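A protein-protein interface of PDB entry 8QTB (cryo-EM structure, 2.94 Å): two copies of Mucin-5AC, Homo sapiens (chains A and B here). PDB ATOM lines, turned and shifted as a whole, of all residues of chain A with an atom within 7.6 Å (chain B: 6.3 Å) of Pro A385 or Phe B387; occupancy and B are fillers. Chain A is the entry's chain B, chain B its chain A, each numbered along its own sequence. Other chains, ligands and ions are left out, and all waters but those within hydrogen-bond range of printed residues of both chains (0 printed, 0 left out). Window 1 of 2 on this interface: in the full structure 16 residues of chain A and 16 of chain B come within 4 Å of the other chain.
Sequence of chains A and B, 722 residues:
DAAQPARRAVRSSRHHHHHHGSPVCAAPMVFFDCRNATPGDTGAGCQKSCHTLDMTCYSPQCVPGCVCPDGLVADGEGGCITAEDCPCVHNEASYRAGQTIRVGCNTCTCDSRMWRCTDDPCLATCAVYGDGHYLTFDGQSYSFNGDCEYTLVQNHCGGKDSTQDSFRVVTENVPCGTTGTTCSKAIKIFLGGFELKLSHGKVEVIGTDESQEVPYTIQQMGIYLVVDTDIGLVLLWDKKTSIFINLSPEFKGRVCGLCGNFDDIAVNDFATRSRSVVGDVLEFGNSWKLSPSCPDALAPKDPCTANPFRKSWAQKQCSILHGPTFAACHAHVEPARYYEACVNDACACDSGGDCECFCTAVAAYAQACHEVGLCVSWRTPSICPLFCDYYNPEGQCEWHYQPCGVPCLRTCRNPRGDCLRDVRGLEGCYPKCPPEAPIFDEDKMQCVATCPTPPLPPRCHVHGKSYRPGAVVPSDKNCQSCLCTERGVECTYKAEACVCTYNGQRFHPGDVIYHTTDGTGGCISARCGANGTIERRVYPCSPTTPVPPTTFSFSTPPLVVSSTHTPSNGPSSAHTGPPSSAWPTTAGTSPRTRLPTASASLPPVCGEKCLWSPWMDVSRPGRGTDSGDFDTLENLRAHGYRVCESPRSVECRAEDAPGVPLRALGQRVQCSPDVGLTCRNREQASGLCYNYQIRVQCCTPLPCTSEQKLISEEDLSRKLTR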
ATOM      1  N   CYS A 355       6.163 -17.373  32.036  1.00  0.00           N
ATOM      2  CA  CYS A 355       4.771 -17.804  32.062  1.00  0.00           C
ATOM      3  C   CYS A 355       4.593 -19.019  32.962  1.00  0.00           C
ATOM      4  O   CYS A 355       3.589 -19.131  33.673  1.00  0.00           O
ATOM      5  CB  CYS A 355       4.290 -18.108  30.644  1.00  0.00           C
ATOM      6  SG  CYS A 355       2.661 -18.883  30.556  1.00  0.00           S
ATOM      7  N   CYS A 359       2.135 -19.088  36.157  1.00  0.00           N
ATOM      8  CA  CYS A 359       1.096 -20.108  36.232  1.00  0.00           C
ATOM      9  C   CYS A 359       1.246 -20.955  37.486  1.00  0.00           C
ATOM     10  O   CYS A 359       0.250 -21.313  38.120  1.00  0.00           O
ATOM     11  CB  CYS A 359       1.128 -20.988  34.983  1.00  0.00           C
ATOM     12  SG  CYS A 359       0.589 -20.172  33.458  1.00  0.00           S
ATOM     13  N   SER A 377     -13.004 -20.848  39.085  1.00  0.00           N
ATOM     14  CA  SER A 377     -12.645 -21.149  37.699  1.00  0.00           C
ATOM     15  C   SER A 377     -11.934 -19.922  37.137  1.00  0.00           C
ATOM     16  O   SER A 377     -12.555 -19.024  36.569  1.00  0.00           O
ATOM     17  CB  SER A 377     -13.878 -21.514  36.882  1.00  0.00           C
ATOM     18  OG  SER A 377     -13.545 -21.717  35.521  1.00  0.00           O
ATOM     19  N   TRP A 378     -10.610 -19.890  37.300  1.00  0.00           N
ATOM     20  CA  TRP A 378      -9.812 -18.738  36.903  1.00  0.00           C
ATOM     21  C   TRP A 378      -9.135 -18.899  35.550  1.00  0.00           C
ATOM     22  O   TRP A 378      -8.800 -17.888  34.923  1.00  0.00           O
ATOM     23  CB  TRP A 378      -8.737 -18.452  37.957  1.00  0.00           C
ATOM     24  CG  TRP A 378      -7.781 -19.589  38.148  1.00  0.00           C
ATOM     25  CD1 TRP A 378      -7.916 -20.634  39.013  1.00  0.00           C
ATOM     26  CD2 TRP A 378      -6.547 -19.800  37.453  1.00  0.00           C
ATOM     27  NE1 TRP A 378      -6.841 -21.482  38.902  1.00  0.00           N
ATOM     28  CE2 TRP A 378      -5.985 -20.992  37.952  1.00  0.00           C
ATOM     29  CE3 TRP A 378      -5.861 -19.096  36.459  1.00  0.00           C
ATOM     30  CZ2 TRP A 378      -4.771 -21.495  37.491  1.00  0.00           C
ATOM     31  CZ3 TRP A 378      -4.656 -19.598  36.002  1.00  0.00           C
ATOM     32  CH2 TRP A 378      -4.123 -20.786  36.519  1.00  0.00           C
ATOM     33  N   ARG A 379      -8.918 -20.129  35.092  1.00  0.00           N
ATOM     34  CA  ARG A 379      -8.189 -20.345  33.849  1.00  0.00           C
ATOM     35  C   ARG A 379      -8.987 -19.830  32.659  1.00  0.00           C
ATOM     36  O   ARG A 379     -10.191 -20.076  32.546  1.00  0.00           O
ATOM     37  CB  ARG A 379      -7.868 -21.828  33.673  1.00  0.00           C
ATOM     38  CG  ARG A 379      -6.900 -22.372  34.709  1.00  0.00           C
ATOM     39  CD  ARG A 379      -6.454 -23.782  34.363  1.00  0.00           C
ATOM     40  NE  ARG A 379      -5.374 -24.238  35.228  1.00  0.00           N
ATOM     41  CZ  ARG A 379      -4.085 -24.051  34.977  1.00  0.00           C
ATOM     42  NH1 ARG A 379      -3.677 -23.421  33.889  1.00  0.00           N
ATOM     43  NH2 ARG A 379      -3.183 -24.509  35.840  1.00  0.00           N
ATOM     44  N   THR A 380      -8.308 -19.112  31.776  1.00  0.00           N
ATOM     45  CA  THR A 380      -8.868 -18.542  30.562  1.00  0.00           C
ATOM     46  C   THR A 380      -7.954 -18.893  29.400  1.00  0.00           C
ATOM     47  O   THR A 380      -6.779 -19.214  29.605  1.00  0.00           O
ATOM     48  CB  THR A 380      -9.011 -17.015  30.670  1.00  0.00           C
ATOM     49  OG1 THR A 380      -7.715 -16.416  30.775  1.00  0.00           O
ATOM     50  CG2 THR A 380      -9.844 -16.636  31.887  1.00  0.00           C
ATOM     51  N   PRO A 381      -8.463 -18.857  28.165  1.00  0.00           N
ATOM     52  CA  PRO A 381      -7.600 -19.172  27.016  1.00  0.00           C
ATOM     53  C   PRO A 381      -6.407 -18.244  26.873  1.00  0.00           C
ATOM     54  O   PRO A 381      -5.410 -18.635  26.257  1.00  0.00           O
ATOM     55  CB  PRO A 381      -8.550 -19.053  25.814  1.00  0.00           C
ATOM     56  CG  PRO A 381      -9.722 -18.269  26.315  1.00  0.00           C
ATOM     57  CD  PRO A 381      -9.860 -18.638  27.754  1.00  0.00           C
ATOM     58  N   SER A 382      -6.476 -17.030  27.417  1.00  0.00           N
ATOM     59  CA  SER A 382      -5.368 -16.089  27.347  1.00  0.00           C
ATOM     60  C   SER A 382      -4.485 -16.095  28.589  1.00  0.00           C
ATOM     61  O   SER A 382      -3.443 -15.432  28.587  1.00  0.00           O
ATOM     62  CB  SER A 382      -5.897 -14.669  27.111  1.00  0.00           C
ATOM     63  OG  SER A 382      -6.717 -14.248  28.187  1.00  0.00           O
ATOM     64  N   ILE A 383      -4.867 -16.817  29.641  1.00  0.00           N
ATOM     65  CA  ILE A 383      -4.107 -16.863  30.888  1.00  0.00           C
ATOM     66  C   ILE A 383      -3.984 -18.320  31.311  1.00  0.00           C
ATOM     67  O   ILE A 383      -4.967 -18.925  31.756  1.00  0.00           O
ATOM     68  CB  ILE A 383      -4.759 -16.031  32.000  1.00  0.00           C
ATOM     69  CG1 ILE A 383      -4.841 -14.558  31.593  1.00  0.00           C
ATOM     70  CG2 ILE A 383      -3.988 -16.183  33.301  1.00  0.00           C
ATOM     71  CD1 ILE A 383      -5.567 -13.691  32.595  1.00  0.00           C
ATOM     72  N   CYS A 384      -2.775 -18.878  31.192  1.00  0.00           N
ATOM     73  CA  CYS A 384      -2.459 -20.249  31.578  1.00  0.00           C
ATOM     74  C   CYS A 384      -3.463 -21.236  30.990  1.00  0.00           C
ATOM     75  O   CYS A 384      -4.212 -21.876  31.740  1.00  0.00           O
ATOM     76  CB  CYS A 384      -2.422 -20.382  33.102  1.00  0.00           C
ATOM     77  SG  CYS A 384      -1.200 -19.334  33.928  1.00  0.00           S
ATOM     78  N   PRO A 385      -3.513 -21.390  29.671  1.00  0.00           N
ATOM     79  CA  PRO A 385      -4.521 -22.261  29.067  1.00  0.00           C
ATOM     80  C   PRO A 385      -4.153 -23.733  29.183  1.00  0.00           C
ATOM     81  O   PRO A 385      -3.007 -24.106  29.440  1.00  0.00           O
ATOM     82  CB  PRO A 385      -4.534 -21.813  27.603  1.00  0.00           C
ATOM     83  CG  PRO A 385      -3.135 -21.363  27.356  1.00  0.00           C
ATOM     84  CD  PRO A 385      -2.609 -20.810  28.662  1.00  0.00           C
ATOM     85  N   LEU A 386      -5.166 -24.574  28.984  1.00  0.00           N
ATOM     86  CA  LEU A 386      -4.997 -26.018  28.944  1.00  0.00           C
ATOM     87  C   LEU A 386      -5.497 -26.536  27.604  1.00  0.00           C
ATOM     88  O   LEU A 386      -6.276 -25.878  26.913  1.00  0.00           O
ATOM     89  CB  LEU A 386      -5.739 -26.713  30.093  1.00  0.00           C
ATOM     90  CG  LEU A 386      -5.378 -26.256  31.505  1.00  0.00           C
ATOM     91  CD1 LEU A 386      -6.263 -26.944  32.530  1.00  0.00           C
ATOM     92  CD2 LEU A 386      -3.909 -26.523  31.792  1.00  0.00           C
ATOM     93  N   PHE A 387      -5.052 -27.737  27.254  1.00  0.00           N
ATOM     94  CA  PHE A 387      -5.262 -28.314  25.928  1.00  0.00           C
ATOM     95  C   PHE A 387      -5.942 -29.671  26.087  1.00  0.00           C
ATOM     96  O   PHE A 387      -5.472 -30.679  25.554  1.00  0.00           O
ATOM     97  CB  PHE A 387      -3.931 -28.430  25.171  1.00  0.00           C
ATOM     98  CG  PHE A 387      -4.089 -28.588  23.685  1.00  0.00           C
ATOM     99  CD1 PHE A 387      -5.313 -28.371  23.076  1.00  0.00           C
ATOM    100  CD2 PHE A 387      -3.009 -28.950  22.896  1.00  0.00           C
ATOM    101  CE1 PHE A 387      -5.459 -28.513  21.710  1.00  0.00           C
ATOM    102  CE2 PHE A 387      -3.149 -29.094  21.530  1.00  0.00           C
ATOM    103  CZ  PHE A 387      -4.376 -28.876  20.936  1.00  0.00           C
ATOM    104  N   CYS A 388      -7.044 -29.690  26.844  1.00  0.00           N
ATOM    105  CA  CYS A 388      -7.753 -30.939  27.114  1.00  0.00           C
ATOM    106  C   CYS A 388      -8.154 -31.651  25.827  1.00  0.00           C
ATOM    107  O   CYS A 388      -8.238 -32.884  25.794  1.00  0.00           O
ATOM    108  CB  CYS A 388      -8.988 -30.661  27.972  1.00  0.00           C
ATOM    109  SG  CYS A 388      -8.649 -29.901  29.578  1.00  0.00           S
ATOM    110  N   ASP A 389      -8.407 -30.895  24.756  1.00  0.00           N
ATOM    111  CA  ASP A 389      -8.815 -31.499  23.492  1.00  0.00           C
ATOM    112  C   ASP A 389      -7.718 -32.354  22.872  1.00  0.00           C
ATOM    113  O   ASP A 389      -8.010 -33.189  22.009  1.00  0.00           O
ATOM    114  CB  ASP A 389      -9.240 -30.409  22.506  1.00  0.00           C
ATOM    115  CG  ASP A 389      -9.981 -30.965  21.306  1.00  0.00           C
ATOM    116  OD1 ASP A 389     -10.544 -32.075  21.413  1.00  0.00           O
ATOM    117  OD2 ASP A 389      -9.999 -30.293  20.253  1.00  0.00           O
ATOM    118  N   HIS A 400     -12.889 -32.835  29.411  1.00  0.00           N
ATOM    119  CA  HIS A 400     -13.291 -31.488  29.785  1.00  0.00           C
ATOM    120  C   HIS A 400     -12.422 -31.009  30.939  1.00  0.00           C
ATOM    121  O   HIS A 400     -11.744 -31.797  31.602  1.00  0.00           O
ATOM    122  CB  HIS A 400     -14.773 -31.422  30.181  1.00  0.00           C
ATOM    123  CG  HIS A 400     -15.713 -31.741  29.061  1.00  0.00           C
ATOM    124  ND1 HIS A 400     -15.996 -33.032  28.671  1.00  0.00           N
ATOM    125  CD2 HIS A 400     -16.435 -30.934  28.248  1.00  0.00           C
ATOM    126  CE1 HIS A 400     -16.853 -33.007  27.666  1.00  0.00           C
ATOM    127  NE2 HIS A 400     -17.135 -31.746  27.390  1.00  0.00           N
ATOM    128  N   TYR A 401     -12.452 -29.700  31.170  1.00  0.00           N
ATOM    129  CA  TYR A 401     -11.692 -29.086  32.251  1.00  0.00           C
ATOM    130  C   TYR A 401     -12.604 -28.885  33.455  1.00  0.00           C
ATOM    131  O   TYR A 401     -13.607 -28.168  33.368  1.00  0.00           O
ATOM    132  CB  TYR A 401     -11.094 -27.753  31.802  1.00  0.00           C
ATOM    133  CG  TYR A 401     -10.709 -26.842  32.944  1.00  0.00           C
ATOM    134  CD1 TYR A 401      -9.705 -27.198  33.833  1.00  0.00           C
ATOM    135  CD2 TYR A 401     -11.349 -25.625  33.133  1.00  0.00           C
ATOM    136  CE1 TYR A 401      -9.349 -26.367  34.878  1.00  0.00           C
ATOM    137  CE2 TYR A 401     -11.001 -24.789  34.175  1.00  0.00           C
ATOM    138  CZ  TYR A 401     -10.001 -25.165  35.045  1.00  0.00           C
ATOM    139  OH  TYR A 401      -9.650 -24.335  36.085  1.00  0.00           O
ATOM    140  N   CYS A 429      -7.554 -31.563  33.260  1.00  0.00           N
ATOM    141  CA  CYS A 429      -8.420 -32.259  32.318  1.00  0.00           C
ATOM    142  C   CYS A 429      -8.817 -33.619  32.880  1.00  0.00           C
ATOM    143  O   CYS A 429      -7.975 -34.358  33.399  1.00  0.00           O
ATOM    144  CB  CYS A 429      -7.715 -32.428  30.973  1.00  0.00           C
ATOM    145  SG  CYS A 429      -7.030 -30.904  30.284  1.00  0.00           S
ATOM    146  N   PRO B 381       0.145 -29.825  24.008  1.00  0.00           N
ATOM    147  CA  PRO B 381      -0.265 -29.198  25.277  1.00  0.00           C
ATOM    148  C   PRO B 381       0.874 -28.524  26.021  1.00  0.00           C
ATOM    149  O   PRO B 381       0.614 -27.624  26.829  1.00  0.00           O
ATOM    150  CB  PRO B 381      -0.842 -30.372  26.083  1.00  0.00           C
ATOM    151  CG  PRO B 381      -0.323 -31.605  25.412  1.00  0.00           C
ATOM    152  CD  PRO B 381      -0.211 -31.253  23.966  1.00  0.00           C
ATOM    153  N   PRO B 385      -0.140 -24.079  23.712  1.00  0.00           N
ATOM    154  CA  PRO B 385      -1.423 -24.786  23.726  1.00  0.00           C
ATOM    155  C   PRO B 385      -2.590 -23.864  23.404  1.00  0.00           C
ATOM    156  O   PRO B 385      -2.496 -22.637  23.468  1.00  0.00           O
ATOM    157  CB  PRO B 385      -1.516 -25.308  25.162  1.00  0.00           C
ATOM    158  CG  PRO B 385      -0.779 -24.288  25.960  1.00  0.00           C
ATOM    159  CD  PRO B 385       0.309 -23.728  25.072  1.00  0.00           C
ATOM    160  N   LEU B 386      -3.710 -24.491  23.052  1.00  0.00           N
ATOM    161  CA  LEU B 386      -4.963 -23.795  22.813  1.00  0.00           C
ATOM    162  C   LEU B 386      -6.025 -24.354  23.750  1.00  0.00           C
ATOM    163  O   LEU B 386      -5.900 -25.463  24.272  1.00  0.00           O
ATOM    164  CB  LEU B 386      -5.423 -23.924  21.356  1.00  0.00           C
ATOM    165  CG  LEU B 386      -4.432 -23.451  20.292  1.00  0.00           C
ATOM    166  CD1 LEU B 386      -4.969 -23.741  18.900  1.00  0.00           C
ATOM    167  CD2 LEU B 386      -4.139 -21.969  20.460  1.00  0.00           C
ATOM    168  N   PHE B 387      -7.083 -23.575  23.943  1.00  0.00           N
ATOM    169  CA  PHE B 387      -8.105 -23.848  24.952  1.00  0.00           C
ATOM    170  C   PHE B 387      -9.468 -23.898  24.264  1.00  0.00           C
ATOM    171  O   PHE B 387     -10.408 -23.214  24.678  1.00  0.00           O
ATOM    172  CB  PHE B 387      -8.066 -22.790  26.063  1.00  0.00           C
ATOM    173  CG  PHE B 387      -8.752 -23.214  27.331  1.00  0.00           C
ATOM    174  CD1 PHE B 387      -9.125 -24.532  27.525  1.00  0.00           C
ATOM    175  CD2 PHE B 387      -9.018 -22.293  28.330  1.00  0.00           C
ATOM    176  CE1 PHE B 387      -9.754 -24.925  28.692  1.00  0.00           C
ATOM    177  CE2 PHE B 387      -9.646 -22.679  29.498  1.00  0.00           C
ATOM    178  CZ  PHE B 387     -10.015 -23.996  29.679  1.00  0.00           C
ATOM    179  N   CYS B 388      -9.559 -24.700  23.199  1.00  0.00           N
ATOM    180  CA  CYS B 388     -10.796 -24.791  22.427  1.00  0.00           C
ATOM    181  C   CYS B 388     -11.983 -25.173  23.304  1.00  0.00           C
ATOM    182  O   CYS B 388     -13.123 -24.782  23.023  1.00  0.00           O
ATOM    183  CB  CYS B 388     -10.629 -25.803  21.292  1.00  0.00           C
ATOM    184  SG  CYS B 388      -9.311 -25.420  20.115  1.00  0.00           S
ATOM    185  N   ASP B 389     -11.741 -25.939  24.371  1.00  0.00           N
ATOM    186  CA  ASP B 389     -12.826 -26.364  25.250  1.00  0.00           C
ATOM    187  C   ASP B 389     -13.471 -25.198  25.988  1.00  0.00           C
ATOM    188  O   ASP B 389     -14.594 -25.338  26.487  1.00  0.00           O
ATOM    189  CB  ASP B 389     -12.307 -27.391  26.259  1.00  0.00           C
ATOM    190  CG  ASP B 389     -13.428 -28.118  26.979  1.00  0.00           C
ATOM    191  OD1 ASP B 389     -14.551 -28.169  26.436  1.00  0.00           O
ATOM    192  OD2 ASP B 389     -13.184 -28.635  28.089  1.00  0.00           O
ATOM    193  N   TYR B 390     -12.789 -24.054  26.076  1.00  0.00           N
ATOM    194  CA  TYR B 390     -13.351 -22.911  26.790  1.00  0.00           C
ATOM    195  C   TYR B 390     -14.628 -22.413  26.125  1.00  0.00           C
ATOM    196  O   TYR B 390     -15.603 -22.079  26.808  1.00  0.00           O
ATOM    197  CB  TYR B 390     -12.317 -21.788  26.875  1.00  0.00           C
ATOM    198  CG  TYR B 390     -12.801 -20.560  27.609  1.00  0.00           C
ATOM    199  CD1 TYR B 390     -12.809 -20.513  28.996  1.00  0.00           C
ATOM    200  CD2 TYR B 390     -13.244 -19.444  26.913  1.00  0.00           C
ATOM    201  CE1 TYR B 390     -13.248 -19.390  29.669  1.00  0.00           C
ATOM    202  CE2 TYR B 390     -13.685 -18.316  27.579  1.00  0.00           C
ATOM    203  CZ  TYR B 390     -13.685 -18.295  28.955  1.00  0.00           C
ATOM    204  OH  TYR B 390     -14.124 -17.174  29.620  1.00  0.00           O
ATOM    205  N   TYR B 391     -14.643 -22.356  24.792  1.00  0.00           N
ATOM    206  CA  TYR B 391     -15.821 -21.875  24.082  1.00  0.00           C
ATOM    207  C   TYR B 391     -16.966 -22.878  24.103  1.00  0.00           C
ATOM    208  O   TYR B 391     -18.090 -22.522  23.733  1.00  0.00           O
ATOM    209  CB  TYR B 391     -15.460 -21.532  22.636  1.00  0.00           C
ATOM    210  CG  TYR B 391     -14.203 -20.705  22.497  1.00  0.00           C
ATOM    211  CD1 TYR B 391     -14.203 -19.349  22.793  1.00  0.00           C
ATOM    212  CD2 TYR B 391     -13.015 -21.280  22.068  1.00  0.00           C
ATOM    213  CE1 TYR B 391     -13.056 -18.590  22.667  1.00  0.00           C
ATOM    214  CE2 TYR B 391     -11.863 -20.528  21.937  1.00  0.00           C
ATOM    215  CZ  TYR B 391     -11.890 -19.184  22.238  1.00  0.00           C
ATOM    216  OH  TYR B 391     -10.746 -18.433  22.110  1.00  0.00           O
ATOM    217  N   CYS B 429      -9.239 -22.951  16.738  1.00  0.00           N
ATOM    218  CA  CYS B 429     -10.434 -23.674  17.146  1.00  0.00           C
ATOM    219  C   CYS B 429     -11.580 -23.376  16.187  1.00  0.00           C
ATOM    220  O   CYS B 429     -11.817 -22.220  15.825  1.00  0.00           O
ATOM    221  CB  CYS B 429     -10.825 -23.292  18.572  1.00  0.00           C
ATOM    222  SG  CYS B 429      -9.490 -23.424  19.782  1.00  0.00           S
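Along chain A the printed residues that touch a printed residue of chain B span positions 380 to 401.
Among the printed residues, no Asp or Glu carboxylate lies within 4 Å of a Lys or Arg side-chain nitrogen of the other chain.
The backbone carbonyl oxygen (O) of Leu B386 sits close to the backbone carbonyl oxygen (O) of Leu A386.
The backbone NH (N) of Tyr A401 sits at hydrogen-bond distance from the side-chain carboxylate (OD2) of Asp B389 (3.3 Å).
Thr A380 touches Phe B387.
N of Pro A381 touches CD2 of Phe B387 (3.5 Å).
Tyr B390 touches Pro A381 (CG to CD, 3.5 Å).
CB of Phe B387 touches CB of Pro A385, at 3.98 Å.
Leu A386 touches Phe B387 (O to CD1, 3.2 Å).
Phe A387 touches Pro B381.
Phe A387 touches Pro B385.
Phe A387 touches Leu B386 (CD1 to O, 3.2 Å).
CA of His A400 touches OD2 of Asp B389 (3.3 Å).
Of the printed residues of chain B, Pro A385 touches Phe B387 (3.98 Å).
Of the printed residues of chain B, Phe A387 touches Pro B381 (3.5 Å), Pro B385 (3.9 Å) and Leu B386 (3.2 Å).
Cys A388 touches none of the printed residues of chain B.
Asp A389 touches none of the printed residues of chain B.
Printed residues of chain A within 4 Å of Leu B386: Leu A386 and Phe A387.
Phe B387 touches just these residues of chain A: Thr A380 (3.7 Å), Pro A381 (3.5 Å), Pro A385 (3.98 Å) and Leu A386 (3.2 Å).
Printed residues of chain A within 4 Å of Asp B389: His A400 and Tyr A401.
Pro A381 touches Phe B387, and with the chains exchanged Phe A387 touches Pro B381.
Pro A385 touches Phe B387, and with the chains exchanged Phe A387 touches Pro B385.
Leu A386 touches its own counterpart, Leu B386.
Leu A386 touches Phe B387, and with the chains exchanged Phe A387 touches Leu B386.
Of the 11 pairs that touch across the chains among the printed residues, 7 have their exchanged pair printed and touching as well.
OG1 of Thr A380 lies within hydrogen-bond range of N of Ile A383, at 3.1 Å.
The side-chain sulfur of Cys B388 is disulfide-bonded to the side-chain sulfur of Cys B429.
The side-chain sulfur (SG) of Cys A359 is disulfide-bonded to the side-chain sulfur (SG) of Cys A384 (2.0 Å).
The side-chain sulfur of Cys A388 forms a disulfide with the side-chain sulfur of Cys A429, at 2.0 Å.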
